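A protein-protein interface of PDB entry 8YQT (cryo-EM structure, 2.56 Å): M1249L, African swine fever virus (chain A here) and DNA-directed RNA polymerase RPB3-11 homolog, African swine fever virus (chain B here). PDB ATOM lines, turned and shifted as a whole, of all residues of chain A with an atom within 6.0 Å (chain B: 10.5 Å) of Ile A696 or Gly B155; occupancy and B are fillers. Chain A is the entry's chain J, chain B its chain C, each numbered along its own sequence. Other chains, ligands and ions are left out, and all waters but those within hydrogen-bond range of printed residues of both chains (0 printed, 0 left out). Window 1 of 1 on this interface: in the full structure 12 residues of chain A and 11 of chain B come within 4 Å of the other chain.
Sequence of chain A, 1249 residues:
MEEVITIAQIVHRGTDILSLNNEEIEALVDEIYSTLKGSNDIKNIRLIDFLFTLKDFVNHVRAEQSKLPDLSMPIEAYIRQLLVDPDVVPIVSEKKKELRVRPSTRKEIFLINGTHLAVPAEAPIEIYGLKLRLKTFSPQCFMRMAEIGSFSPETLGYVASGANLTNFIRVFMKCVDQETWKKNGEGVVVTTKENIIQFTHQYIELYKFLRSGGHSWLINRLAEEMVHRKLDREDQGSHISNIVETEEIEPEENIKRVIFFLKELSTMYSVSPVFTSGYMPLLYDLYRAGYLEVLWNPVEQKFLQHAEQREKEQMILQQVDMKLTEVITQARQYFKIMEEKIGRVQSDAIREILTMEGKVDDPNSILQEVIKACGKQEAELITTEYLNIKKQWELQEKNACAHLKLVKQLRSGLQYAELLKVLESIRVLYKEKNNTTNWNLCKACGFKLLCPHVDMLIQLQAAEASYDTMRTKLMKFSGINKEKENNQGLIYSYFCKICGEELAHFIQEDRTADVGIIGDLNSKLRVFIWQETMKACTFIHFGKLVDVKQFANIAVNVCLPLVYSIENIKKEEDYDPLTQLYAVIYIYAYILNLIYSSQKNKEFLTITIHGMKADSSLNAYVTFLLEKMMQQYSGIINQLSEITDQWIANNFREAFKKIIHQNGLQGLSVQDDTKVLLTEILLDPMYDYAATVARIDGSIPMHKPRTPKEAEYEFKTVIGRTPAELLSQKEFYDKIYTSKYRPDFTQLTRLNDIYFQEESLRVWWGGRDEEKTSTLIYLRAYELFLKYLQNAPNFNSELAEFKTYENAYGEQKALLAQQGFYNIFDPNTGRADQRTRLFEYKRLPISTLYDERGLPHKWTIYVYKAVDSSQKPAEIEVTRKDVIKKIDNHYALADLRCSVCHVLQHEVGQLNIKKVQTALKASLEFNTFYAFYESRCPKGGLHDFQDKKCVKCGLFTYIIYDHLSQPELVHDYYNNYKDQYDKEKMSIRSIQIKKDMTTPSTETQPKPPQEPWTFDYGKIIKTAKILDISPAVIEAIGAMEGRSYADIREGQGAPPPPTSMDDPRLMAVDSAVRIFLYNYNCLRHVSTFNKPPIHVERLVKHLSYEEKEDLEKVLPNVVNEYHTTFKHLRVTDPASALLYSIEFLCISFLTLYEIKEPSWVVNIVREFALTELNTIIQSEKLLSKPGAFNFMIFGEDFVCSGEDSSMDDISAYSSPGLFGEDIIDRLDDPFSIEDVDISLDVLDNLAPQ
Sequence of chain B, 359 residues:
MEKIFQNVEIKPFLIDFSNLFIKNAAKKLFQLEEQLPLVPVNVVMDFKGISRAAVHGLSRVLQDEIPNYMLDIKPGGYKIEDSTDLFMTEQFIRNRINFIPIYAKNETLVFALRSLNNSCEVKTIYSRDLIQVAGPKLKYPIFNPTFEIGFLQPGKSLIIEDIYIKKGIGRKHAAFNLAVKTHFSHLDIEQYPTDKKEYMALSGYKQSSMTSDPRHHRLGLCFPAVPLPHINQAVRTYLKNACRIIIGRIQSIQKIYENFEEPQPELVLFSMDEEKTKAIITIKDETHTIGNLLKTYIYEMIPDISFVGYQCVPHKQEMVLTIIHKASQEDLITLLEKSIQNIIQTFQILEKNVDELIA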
ATOM      1  N   ALA A 691      15.997  15.178  -6.602  1.00  0.00           N
ATOM      2  CA  ALA A 691      16.199  14.573  -7.912  1.00  0.00           C
ATOM      3  C   ALA A 691      17.628  14.755  -8.404  1.00  0.00           C
ATOM      4  O   ALA A 691      18.188  13.843  -9.017  1.00  0.00           O
ATOM      5  CB  ALA A 691      15.212  15.156  -8.920  1.00  0.00           C
ATOM      6  N   THR A 692      18.227  15.923  -8.164  1.00  0.00           N
ATOM      7  CA  THR A 692      19.626  16.122  -8.526  1.00  0.00           C
ATOM      8  C   THR A 692      20.526  15.157  -7.764  1.00  0.00           C
ATOM      9  O   THR A 692      21.421  14.526  -8.346  1.00  0.00           O
ATOM     10  CB  THR A 692      20.039  17.569  -8.253  1.00  0.00           C
ATOM     11  OG1 THR A 692      19.298  18.450  -9.104  1.00  0.00           O
ATOM     12  CG2 THR A 692      21.518  17.753  -8.511  1.00  0.00           C
ATOM     13  N   VAL A 693      20.294  15.023  -6.456  1.00  0.00           N
ATOM     14  CA  VAL A 693      21.096  14.101  -5.658  1.00  0.00           C
ATOM     15  C   VAL A 693      20.919  12.668  -6.149  1.00  0.00           C
ATOM     16  O   VAL A 693      21.880  11.890  -6.171  1.00  0.00           O
ATOM     17  CB  VAL A 693      20.744  14.245  -4.165  1.00  0.00           C
ATOM     18  CG1 VAL A 693      21.464  13.195  -3.341  1.00  0.00           C
ATOM     19  CG2 VAL A 693      21.110  15.630  -3.677  1.00  0.00           C
ATOM     20  N   ALA A 694      19.704  12.301  -6.562  1.00  0.00           N
ATOM     21  CA  ALA A 694      19.470  10.960  -7.089  1.00  0.00           C
ATOM     22  C   ALA A 694      20.136  10.753  -8.445  1.00  0.00           C
ATOM     23  O   ALA A 694      20.611   9.650  -8.735  1.00  0.00           O
ATOM     24  CB  ALA A 694      17.969  10.692  -7.190  1.00  0.00           C
ATOM     25  N   ARG A 695      20.167  11.787  -9.288  1.00  0.00           N
ATOM     26  CA  ARG A 695      20.849  11.684 -10.575  1.00  0.00           C
ATOM     27  C   ARG A 695      22.354  11.548 -10.407  1.00  0.00           C
ATOM     28  O   ARG A 695      23.004  10.872 -11.211  1.00  0.00           O
ATOM     29  CB  ARG A 695      20.543  12.902 -11.448  1.00  0.00           C
ATOM     30  CG  ARG A 695      19.172  12.897 -12.076  1.00  0.00           C
ATOM     31  CD  ARG A 695      18.996  14.052 -13.043  1.00  0.00           C
ATOM     32  NE  ARG A 695      17.619  14.149 -13.511  1.00  0.00           N
ATOM     33  CZ  ARG A 695      16.703  14.945 -12.978  1.00  0.00           C
ATOM     34  NH1 ARG A 695      16.991  15.748 -11.967  1.00  0.00           N
ATOM     35  NH2 ARG A 695      15.469  14.936 -13.470  1.00  0.00           N
ATOM     36  N   ILE A 696      22.924  12.193  -9.388  1.00  0.00           N
ATOM     37  CA  ILE A 696      24.376  12.176  -9.215  1.00  0.00           C
ATOM     38  C   ILE A 696      24.881  10.749  -9.044  1.00  0.00           C
ATOM     39  O   ILE A 696      25.887  10.351  -9.644  1.00  0.00           O
ATOM     40  CB  ILE A 696      24.784  13.071  -8.032  1.00  0.00           C
ATOM     41  CG1 ILE A 696      24.767  14.540  -8.458  1.00  0.00           C
ATOM     42  CG2 ILE A 696      26.149  12.672  -7.504  1.00  0.00           C
ATOM     43  CD1 ILE A 696      24.929  15.509  -7.319  1.00  0.00           C
ATOM     44  N   ASP A 697      24.185   9.947  -8.239  1.00  0.00           N
ATOM     45  CA  ASP A 697      24.597   8.574  -7.971  1.00  0.00           C
ATOM     46  C   ASP A 697      23.769   7.551  -8.747  1.00  0.00           C
ATOM     47  O   ASP A 697      23.729   6.373  -8.374  1.00  0.00           O
ATOM     48  CB  ASP A 697      24.548   8.290  -6.471  1.00  0.00           C
ATOM     49  CG  ASP A 697      23.258   8.741  -5.836  1.00  0.00           C
ATOM     50  OD1 ASP A 697      22.363   9.200  -6.572  1.00  0.00           O
ATOM     51  OD2 ASP A 697      23.136   8.643  -4.597  1.00  0.00           O
ATOM     52  N   GLY A 698      23.102   7.980  -9.816  1.00  0.00           N
ATOM     53  CA  GLY A 698      22.515   7.062 -10.772  1.00  0.00           C
ATOM     54  C   GLY A 698      21.207   6.419 -10.375  1.00  0.00           C
ATOM     55  O   GLY A 698      20.798   5.448 -11.020  1.00  0.00           O
ATOM     56  N   SER A 699      20.531   6.922  -9.341  1.00  0.00           N
ATOM     57  CA  SER A 699      19.270   6.316  -8.927  1.00  0.00           C
ATOM     58  C   SER A 699      18.138   6.612  -9.904  1.00  0.00           C
ATOM     59  O   SER A 699      17.184   5.833  -9.993  1.00  0.00           O
ATOM     60  CB  SER A 699      18.894   6.794  -7.526  1.00  0.00           C
ATOM     61  OG  SER A 699      19.820   6.318  -6.566  1.00  0.00           O
ATOM     62  N   MET A 702      19.507  10.481 -16.099  1.00  0.00           N
ATOM     63  CA  MET A 702      20.063  11.828 -16.149  1.00  0.00           C
ATOM     64  C   MET A 702      19.184  12.804 -16.918  1.00  0.00           C
ATOM     65  O   MET A 702      19.363  14.018 -16.780  1.00  0.00           O
ATOM     66  CB  MET A 702      21.454  11.793 -16.772  1.00  0.00           C
ATOM     67  CG  MET A 702      22.436  12.705 -16.088  1.00  0.00           C
ATOM     68  SD  MET A 702      23.178  11.880 -14.677  1.00  0.00           S
ATOM     69  CE  MET A 702      24.055  13.241 -13.938  1.00  0.00           C
ATOM     70  N   TYR A 741      26.129   7.528  -1.320  1.00  0.00           N
ATOM     71  CA  TYR A 741      27.436   7.512  -0.670  1.00  0.00           C
ATOM     72  C   TYR A 741      27.429   8.367   0.551  1.00  0.00           C
ATOM     73  O   TYR A 741      27.099   9.538   0.487  1.00  0.00           O
ATOM     74  CB  TYR A 741      28.598   7.883  -1.574  1.00  0.00           C
ATOM     75  CG  TYR A 741      28.415   8.957  -2.601  1.00  0.00           C
ATOM     76  CD1 TYR A 741      29.314   9.055  -3.648  1.00  0.00           C
ATOM     77  CD2 TYR A 741      27.395   9.883  -2.524  1.00  0.00           C
ATOM     78  CE1 TYR A 741      29.195  10.029  -4.604  1.00  0.00           C
ATOM     79  CE2 TYR A 741      27.268  10.869  -3.483  1.00  0.00           C
ATOM     80  CZ  TYR A 741      28.177  10.931  -4.516  1.00  0.00           C
ATOM     81  OH  TYR A 741      28.089  11.895  -5.483  1.00  0.00           O
ATOM     82  N   TYR A 778      28.857  19.269  -0.644  1.00  0.00           N
ATOM     83  CA  TYR A 778      27.569  19.111  -1.315  1.00  0.00           C
ATOM     84  C   TYR A 778      26.700  18.070  -0.615  1.00  0.00           C
ATOM     85  O   TYR A 778      25.527  18.327  -0.303  1.00  0.00           O
ATOM     86  CB  TYR A 778      27.801  18.724  -2.777  1.00  0.00           C
ATOM     87  CG  TYR A 778      26.561  18.762  -3.637  1.00  0.00           C
ATOM     88  CD1 TYR A 778      26.189  19.920  -4.300  1.00  0.00           C
ATOM     89  CD2 TYR A 778      25.760  17.639  -3.781  1.00  0.00           C
ATOM     90  CE1 TYR A 778      25.059  19.960  -5.083  1.00  0.00           C
ATOM     91  CE2 TYR A 778      24.624  17.671  -4.559  1.00  0.00           C
ATOM     92  CZ  TYR A 778      24.280  18.834  -5.208  1.00  0.00           C
ATOM     93  OH  TYR A 778      23.151  18.870  -5.988  1.00  0.00           O
ATOM     94  N   LEU A 779      27.259  16.882  -0.368  1.00  0.00           N
ATOM     95  CA  LEU A 779      26.476  15.812   0.238  1.00  0.00           C
ATOM     96  C   LEU A 779      26.060  16.150   1.662  1.00  0.00           C
ATOM     97  O   LEU A 779      24.921  15.874   2.051  1.00  0.00           O
ATOM     98  CB  LEU A 779      27.261  14.503   0.211  1.00  0.00           C
ATOM     99  CG  LEU A 779      27.535  13.917  -1.174  1.00  0.00           C
ATOM    100  CD1 LEU A 779      28.410  12.691  -1.053  1.00  0.00           C
ATOM    101  CD2 LEU A 779      26.237  13.583  -1.889  1.00  0.00           C
ATOM    102  N   GLU B  81      15.391  18.326 -24.537  1.00  0.00           N
ATOM    103  CA  GLU B  81      14.954  17.256 -23.648  1.00  0.00           C
ATOM    104  C   GLU B  81      16.120  16.630 -22.895  1.00  0.00           C
ATOM    105  O   GLU B  81      15.961  16.219 -21.741  1.00  0.00           O
ATOM    106  CB  GLU B  81      14.212  16.188 -24.450  1.00  0.00           C
ATOM    107  CG  GLU B  81      12.994  16.706 -25.194  1.00  0.00           C
ATOM    108  CD  GLU B  81      11.829  16.999 -24.273  1.00  0.00           C
ATOM    109  OE1 GLU B  81      11.665  16.270 -23.272  1.00  0.00           O
ATOM    110  OE2 GLU B  81      11.078  17.957 -24.552  1.00  0.00           O
ATOM    111  N   ASP B  82      17.291  16.556 -23.521  1.00  0.00           N
ATOM    112  CA  ASP B  82      18.448  15.893 -22.935  1.00  0.00           C
ATOM    113  C   ASP B  82      19.378  16.836 -22.188  1.00  0.00           C
ATOM    114  O   ASP B  82      20.048  16.403 -21.247  1.00  0.00           O
ATOM    115  CB  ASP B  82      19.242  15.168 -24.024  1.00  0.00           C
ATOM    116  CG  ASP B  82      18.548  13.922 -24.517  1.00  0.00           C
ATOM    117  OD1 ASP B  82      17.881  13.254 -23.701  1.00  0.00           O
ATOM    118  OD2 ASP B  82      18.667  13.613 -25.720  1.00  0.00           O
ATOM    119  N   SER B  83      19.445  18.105 -22.582  1.00  0.00           N
ATOM    120  CA  SER B  83      20.305  19.076 -21.910  1.00  0.00           C
ATOM    121  C   SER B  83      19.565  19.613 -20.695  1.00  0.00           C
ATOM    122  O   SER B  83      18.719  20.501 -20.810  1.00  0.00           O
ATOM    123  CB  SER B  83      20.694  20.203 -22.858  1.00  0.00           C
ATOM    124  OG  SER B  83      21.462  19.714 -23.941  1.00  0.00           O
ATOM    125  N   THR B  84      19.884  19.078 -19.522  1.00  0.00           N
ATOM    126  CA  THR B  84      19.222  19.476 -18.290  1.00  0.00           C
ATOM    127  C   THR B  84      19.901  20.649 -17.597  1.00  0.00           C
ATOM    128  O   THR B  84      19.388  21.124 -16.579  1.00  0.00           O
ATOM    129  CB  THR B  84      19.142  18.292 -17.321  1.00  0.00           C
ATOM    130  OG1 THR B  84      20.462  17.880 -16.955  1.00  0.00           O
ATOM    131  CG2 THR B  84      18.420  17.127 -17.966  1.00  0.00           C
ATOM    132  N   ASP B  85      21.030  21.131 -18.110  1.00  0.00           N
ATOM    133  CA  ASP B  85      21.728  22.229 -17.457  1.00  0.00           C
ATOM    134  C   ASP B  85      20.978  23.532 -17.683  1.00  0.00           C
ATOM    135  O   ASP B  85      20.621  23.869 -18.815  1.00  0.00           O
ATOM    136  CB  ASP B  85      23.159  22.358 -17.966  1.00  0.00           C
ATOM    137  CG  ASP B  85      23.984  23.309 -17.119  1.00  0.00           C
ATOM    138  OD1 ASP B  85      24.444  22.900 -16.035  1.00  0.00           O
ATOM    139  OD2 ASP B  85      24.159  24.475 -17.528  1.00  0.00           O
ATOM    140  N   LEU B  86      20.754  24.267 -16.601  1.00  0.00           N
ATOM    141  CA  LEU B  86      19.955  25.478 -16.646  1.00  0.00           C
ATOM    142  C   LEU B  86      20.759  26.719 -17.008  1.00  0.00           C
ATOM    143  O   LEU B  86      20.162  27.746 -17.345  1.00  0.00           O
ATOM    144  CB  LEU B  86      19.273  25.689 -15.295  1.00  0.00           C
ATOM    145  CG  LEU B  86      18.345  24.582 -14.796  1.00  0.00           C
ATOM    146  CD1 LEU B  86      17.773  24.952 -13.444  1.00  0.00           C
ATOM    147  CD2 LEU B  86      17.238  24.309 -15.794  1.00  0.00           C
ATOM    148  N   SER B 115      27.830  15.531 -22.895  1.00  0.00           N
ATOM    149  CA  SER B 115      28.465  15.702 -21.597  1.00  0.00           C
ATOM    150  C   SER B 115      27.482  15.375 -20.484  1.00  0.00           C
ATOM    151  O   SER B 115      26.360  15.892 -20.467  1.00  0.00           O
ATOM    152  CB  SER B 115      28.989  17.127 -21.435  1.00  0.00           C
ATOM    153  OG  SER B 115      30.065  17.368 -22.320  1.00  0.00           O
ATOM    154  N   LEU B 116      27.913  14.522 -19.559  1.00  0.00           N
ATOM    155  CA  LEU B 116      27.148  14.150 -18.379  1.00  0.00           C
ATOM    156  C   LEU B 116      27.974  14.473 -17.143  1.00  0.00           C
ATOM    157  O   LEU B 116      29.197  14.303 -17.145  1.00  0.00           O
ATOM    158  CB  LEU B 116      26.794  12.656 -18.387  1.00  0.00           C
ATOM    159  CG  LEU B 116      25.727  12.117 -19.346  1.00  0.00           C
ATOM    160  CD1 LEU B 116      24.457  12.928 -19.250  1.00  0.00           C
ATOM    161  CD2 LEU B 116      26.215  12.045 -20.785  1.00  0.00           C
ATOM    162  N   ASN B 117      27.313  14.937 -16.087  1.00  0.00           N
ATOM    163  CA  ASN B 117      27.989  15.304 -14.844  1.00  0.00           C
ATOM    164  C   ASN B 117      27.446  14.433 -13.714  1.00  0.00           C
ATOM    165  O   ASN B 117      26.541  14.838 -12.983  1.00  0.00           O
ATOM    166  CB  ASN B 117      27.809  16.786 -14.543  1.00  0.00           C
ATOM    167  CG  ASN B 117      28.774  17.286 -13.497  1.00  0.00           C
ATOM    168  OD1 ASN B 117      29.618  16.539 -13.012  1.00  0.00           O
ATOM    169  ND2 ASN B 117      28.657  18.557 -13.142  1.00  0.00           N
ATOM    170  N   ASN B 118      28.031  13.247 -13.550  1.00  0.00           N
ATOM    171  CA  ASN B 118      27.634  12.301 -12.518  1.00  0.00           C
ATOM    172  C   ASN B 118      28.314  12.561 -11.180  1.00  0.00           C
ATOM    173  O   ASN B 118      28.385  11.650 -10.347  1.00  0.00           O
ATOM    174  CB  ASN B 118      27.940  10.872 -12.969  1.00  0.00           C
ATOM    175  CG  ASN B 118      26.933  10.343 -13.958  1.00  0.00           C
ATOM    176  OD1 ASN B 118      25.728  10.432 -13.740  1.00  0.00           O
ATOM    177  ND2 ASN B 118      27.421   9.785 -15.058  1.00  0.00           N
ATOM    178  N   SER B 119      28.821  13.767 -10.953  1.00  0.00           N
ATOM    179  CA  SER B 119      29.607  14.057  -9.764  1.00  0.00           C
ATOM    180  C   SER B 119      28.966  15.191  -8.979  1.00  0.00           C
ATOM    181  O   SER B 119      28.042  15.862  -9.445  1.00  0.00           O
ATOM    182  CB  SER B 119      31.057  14.407 -10.124  1.00  0.00           C
ATOM    183  OG  SER B 119      31.126  15.627 -10.839  1.00  0.00           O
ATOM    184  N   CYS B 120      29.471  15.396  -7.767  1.00  0.00           N
ATOM    185  CA  CYS B 120      28.991  16.444  -6.881  1.00  0.00           C
ATOM    186  C   CYS B 120      29.683  17.777  -7.116  1.00  0.00           C
ATOM    187  O   CYS B 120      29.378  18.751  -6.421  1.00  0.00           O
ATOM    188  CB  CYS B 120      29.170  16.020  -5.420  1.00  0.00           C
ATOM    189  SG  CYS B 120      28.222  14.556  -4.950  1.00  0.00           S
ATOM    190  N   GLU B 121      30.605  17.845  -8.068  1.00  0.00           N
ATOM    191  CA  GLU B 121      31.325  19.065  -8.386  1.00  0.00           C
ATOM    192  C   GLU B 121      31.015  19.503  -9.812  1.00  0.00           C
ATOM    193  O   GLU B 121      30.672  18.691 -10.674  1.00  0.00           O
ATOM    194  CB  GLU B 121      32.835  18.874  -8.208  1.00  0.00           C
ATOM    195  CG  GLU B 121      33.416  17.698  -8.974  1.00  0.00           C
ATOM    196  CD  GLU B 121      33.798  16.538  -8.074  1.00  0.00           C
ATOM    197  OE1 GLU B 121      33.383  16.533  -6.896  1.00  0.00           O
ATOM    198  OE2 GLU B 121      34.519  15.632  -8.542  1.00  0.00           O
ATOM    199  N   VAL B 122      31.129  20.811 -10.044  1.00  0.00           N
ATOM    200  CA  VAL B 122      30.898  21.370 -11.370  1.00  0.00           C
ATOM    201  C   VAL B 122      31.930  20.811 -12.340  1.00  0.00           C
ATOM    202  O   VAL B 122      33.125  20.742 -12.029  1.00  0.00           O
ATOM    203  CB  VAL B 122      30.944  22.903 -11.319  1.00  0.00           C
ATOM    204  CG1 VAL B 122      30.937  23.490 -12.716  1.00  0.00           C
ATOM    205  CG2 VAL B 122      29.775  23.434 -10.516  1.00  0.00           C
ATOM    206  N   LYS B 123      31.473  20.401 -13.521  1.00  0.00           N
ATOM    207  CA  LYS B 123      32.326  19.756 -14.508  1.00  0.00           C
ATOM    208  C   LYS B 123      32.460  20.637 -15.741  1.00  0.00           C
ATOM    209  O   LYS B 123      31.460  21.054 -16.323  1.00  0.00           O
ATOM    210  CB  LYS B 123      31.758  18.396 -14.909  1.00  0.00           C
ATOM    211  CG  LYS B 123      32.579  17.646 -15.935  1.00  0.00           C
ATOM    212  CD  LYS B 123      31.864  16.380 -16.369  1.00  0.00           C
ATOM    213  CE  LYS B 123      32.606  15.674 -17.485  1.00  0.00           C
ATOM    214  NZ  LYS B 123      33.888  15.092 -17.010  1.00  0.00           N
ATOM    215  N   PHE B 151      30.365  24.684 -18.703  1.00  0.00           N
ATOM    216  CA  PHE B 151      30.439  23.984 -17.428  1.00  0.00           C
ATOM    217  C   PHE B 151      29.043  23.554 -17.005  1.00  0.00           C
ATOM    218  O   PHE B 151      28.064  24.260 -17.250  1.00  0.00           O
ATOM    219  CB  PHE B 151      31.089  24.842 -16.333  1.00  0.00           C
ATOM    220  CG  PHE B 151      30.482  26.204 -16.174  1.00  0.00           C
ATOM    221  CD1 PHE B 151      29.471  26.424 -15.256  1.00  0.00           C
ATOM    222  CD2 PHE B 151      30.939  27.272 -16.921  1.00  0.00           C
ATOM    223  CE1 PHE B 151      28.921  27.673 -15.102  1.00  0.00           C
ATOM    224  CE2 PHE B 151      30.391  28.524 -16.769  1.00  0.00           C
ATOM    225  CZ  PHE B 151      29.382  28.725 -15.858  1.00  0.00           C
ATOM    226  N   LEU B 152      28.971  22.395 -16.361  1.00  0.00           N
ATOM    227  CA  LEU B 152      27.727  21.779 -15.932  1.00  0.00           C
ATOM    228  C   LEU B 152      27.686  21.711 -14.414  1.00  0.00           C
ATOM    229  O   LEU B 152      28.667  21.305 -13.778  1.00  0.00           O
ATOM    230  CB  LEU B 152      27.582  20.373 -16.511  1.00  0.00           C
ATOM    231  CG  LEU B 152      27.607  20.228 -18.027  1.00  0.00           C
ATOM    232  CD1 LEU B 152      27.665  18.765 -18.405  1.00  0.00           C
ATOM    233  CD2 LEU B 152      26.400  20.896 -18.640  1.00  0.00           C
ATOM    234  N   GLN B 153      26.549  22.099 -13.847  1.00  0.00           N
ATOM    235  CA  GLN B 153      26.304  21.941 -12.429  1.00  0.00           C
ATOM    236  C   GLN B 153      26.187  20.456 -12.093  1.00  0.00           C
ATOM    237  O   GLN B 153      25.947  19.633 -12.977  1.00  0.00           O
ATOM    238  CB  GLN B 153      25.031  22.681 -12.032  1.00  0.00           C
ATOM    239  CG  GLN B 153      25.032  24.150 -12.399  1.00  0.00           C
ATOM    240  CD  GLN B 153      26.149  24.914 -11.730  1.00  0.00           C
ATOM    241  OE1 GLN B 153      26.422  24.725 -10.547  1.00  0.00           O
ATOM    242  NE2 GLN B 153      26.809  25.778 -12.485  1.00  0.00           N
ATOM    243  N   PRO B 154      26.384  20.086 -10.828  1.00  0.00           N
ATOM    244  CA  PRO B 154      26.294  18.669 -10.458  1.00  0.00           C
ATOM    245  C   PRO B 154      24.957  18.066 -10.861  1.00  0.00           C
ATOM    246  O   PRO B 154      23.895  18.626 -10.587  1.00  0.00           O
ATOM    247  CB  PRO B 154      26.466  18.694  -8.937  1.00  0.00           C
ATOM    248  CG  PRO B 154      27.240  19.923  -8.673  1.00  0.00           C
ATOM    249  CD  PRO B 154      26.807  20.923  -9.692  1.00  0.00           C
ATOM    250  N   GLY B 155      25.020  16.911 -11.516  1.00  0.00           N
ATOM    251  CA  GLY B 155      23.830  16.206 -11.938  1.00  0.00           C
ATOM    252  C   GLY B 155      23.214  16.666 -13.239  1.00  0.00           C
ATOM    253  O   GLY B 155      22.134  16.183 -13.593  1.00  0.00           O
ATOM    254  N   LYS B 156      23.859  17.571 -13.966  1.00  0.00           N
ATOM    255  CA  LYS B 156      23.298  18.146 -15.178  1.00  0.00           C
ATOM    256  C   LYS B 156      23.930  17.521 -16.414  1.00  0.00           C
ATOM    257  O   LYS B 156      24.887  16.749 -16.336  1.00  0.00           O
ATOM    258  CB  LYS B 156      23.484  19.666 -15.189  1.00  0.00           C
ATOM    259  CG  LYS B 156      22.826  20.359 -14.016  1.00  0.00           C
ATOM    260  CD  LYS B 156      21.338  20.092 -14.004  1.00  0.00           C
ATOM    261  CE  LYS B 156      20.656  20.817 -12.863  1.00  0.00           C
ATOM    262  NZ  LYS B 156      19.190  20.579 -12.867  1.00  0.00           N
ATOM    263  N   SER B 157      23.374  17.873 -17.571  1.00  0.00           N
ATOM    264  CA  SER B 157      23.772  17.282 -18.838  1.00  0.00           C
ATOM    265  C   SER B 157      23.787  18.350 -19.919  1.00  0.00           C
ATOM    266  O   SER B 157      23.207  19.427 -19.769  1.00  0.00           O
ATOM    267  CB  SER B 157      22.829  16.148 -19.247  1.00  0.00           C
ATOM    268  OG  SER B 157      22.635  15.243 -18.178  1.00  0.00           O
ATOM    269  N   LEU B 158      24.471  18.038 -21.018  1.00  0.00           N
ATOM    270  CA  LEU B 158      24.463  18.897 -22.200  1.00  0.00           C
ATOM    271  C   LEU B 158      24.667  18.010 -23.418  1.00  0.00           C
ATOM    272  O   LEU B 158      25.751  17.450 -23.604  1.00  0.00           O
ATOM    273  CB  LEU B 158      25.537  19.976 -22.116  1.00  0.00           C
ATOM    274  CG  LEU B 158      25.514  21.039 -23.218  1.00  0.00           C
ATOM    275  CD1 LEU B 158      24.201  21.793 -23.213  1.00  0.00           C
ATOM    276  CD2 LEU B 158      26.674  22.002 -23.073  1.00  0.00           C
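Arg A695 touches Asn B118 (O to OD1, 3.7 Å).
Arg A695 touches Gly B155 (CD to O, 3.8 Å).
Ile A696 touches Ser B119 (CG1 to O, 3.7 Å).
Cys B120 touches Ile A696.
CG1 of Ile A696 touches N of Gly B155, 3.9 Å away.
Met A702 touches Leu B116.
O of Gly B155 touches CE of Met A702, at 3.5 Å.
Ser B157 touches Met A702.
CG of Tyr A778 touches O of Cys B120, 3.96 Å away.
Leu A779 touches Cys B120 (CD2 to SG, 3.8 Å).
Of chain B, only Pro B154 comes within 4 Å of Thr A692.
No residue of chain B comes within 4 Å of Ala A694.
Of the printed residues of chain B, Arg A695 touches Asn B118 (3.7 Å) and Gly B155 (3.8 Å).
Of the printed residues of chain B, Ile A696 touches Asn B118 (2.9 Å), Ser B119 (3.7 Å), Cys B120 (3.8 Å), Pro B154 (3.9 Å) and Gly B155 (3.9 Å).
No residue of chain B comes within 4 Å of Asp A697.
Of the printed residues of chain B, Tyr A778 touches Cys B120 (3.96 Å).
Of the printed residues of chain A, Leu B116 touches Met A702.
Gly B155 touches three residues of chain A.
Of the printed residues of chain A, Ser B157 touches Met A702 (3.3 Å).
The nearest residue of chain B that does not touch Ile A696 is Asn B117 (4.9 Å).
The nearest printed residue of chain A that does not touch Thr B84 is Arg A695 (5.4 Å).
OG of Ser B119 is in hydrogen-bond range of OD1 of Asn B117 (2.8 Å).
The backbone carbonyl oxygen (O) of Glu B121 is in hydrogen-bond range of the side-chain amide nitrogen (ND2) of Asn B117 (3.2 Å).
ND2 of Asn B117 lies within hydrogen-bond range of O of Leu B152 (2.8 Å).
The side-chain amide nitrogen of Asn B117 sits at hydrogen-bond distance from the backbone carbonyl oxygen of Gln B153, at 2.9 Å.
The backbone carbonyl oxygen (O) of Asn B117 is in hydrogen-bond range of the backbone NH (N) of Gly B155 (3.0 Å).
N of Asn B117 is in hydrogen-bond range of O of Lys B156 (3.0 Å).
The side-chain sulfur of Met A702 sits close to the side-chain amide oxygen of Asn B118, 3.1 Å away.
The side-chain sulfur of Cys B120 sits at hydrogen-bond distance from the side-chain hydroxyl of Tyr A741, at 2.7 Å.
The backbone carbonyl oxygen of Ile A696 sits close to the backbone carbonyl oxygen of Asn B118.
Of the 23 printed residues of chain B, 9 touch a printed residue of chain A.
Among the printed residues, no Asp or Glu carboxylate lies within 4 Å of a Lys or Arg side-chain nitrogen of the other chain.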
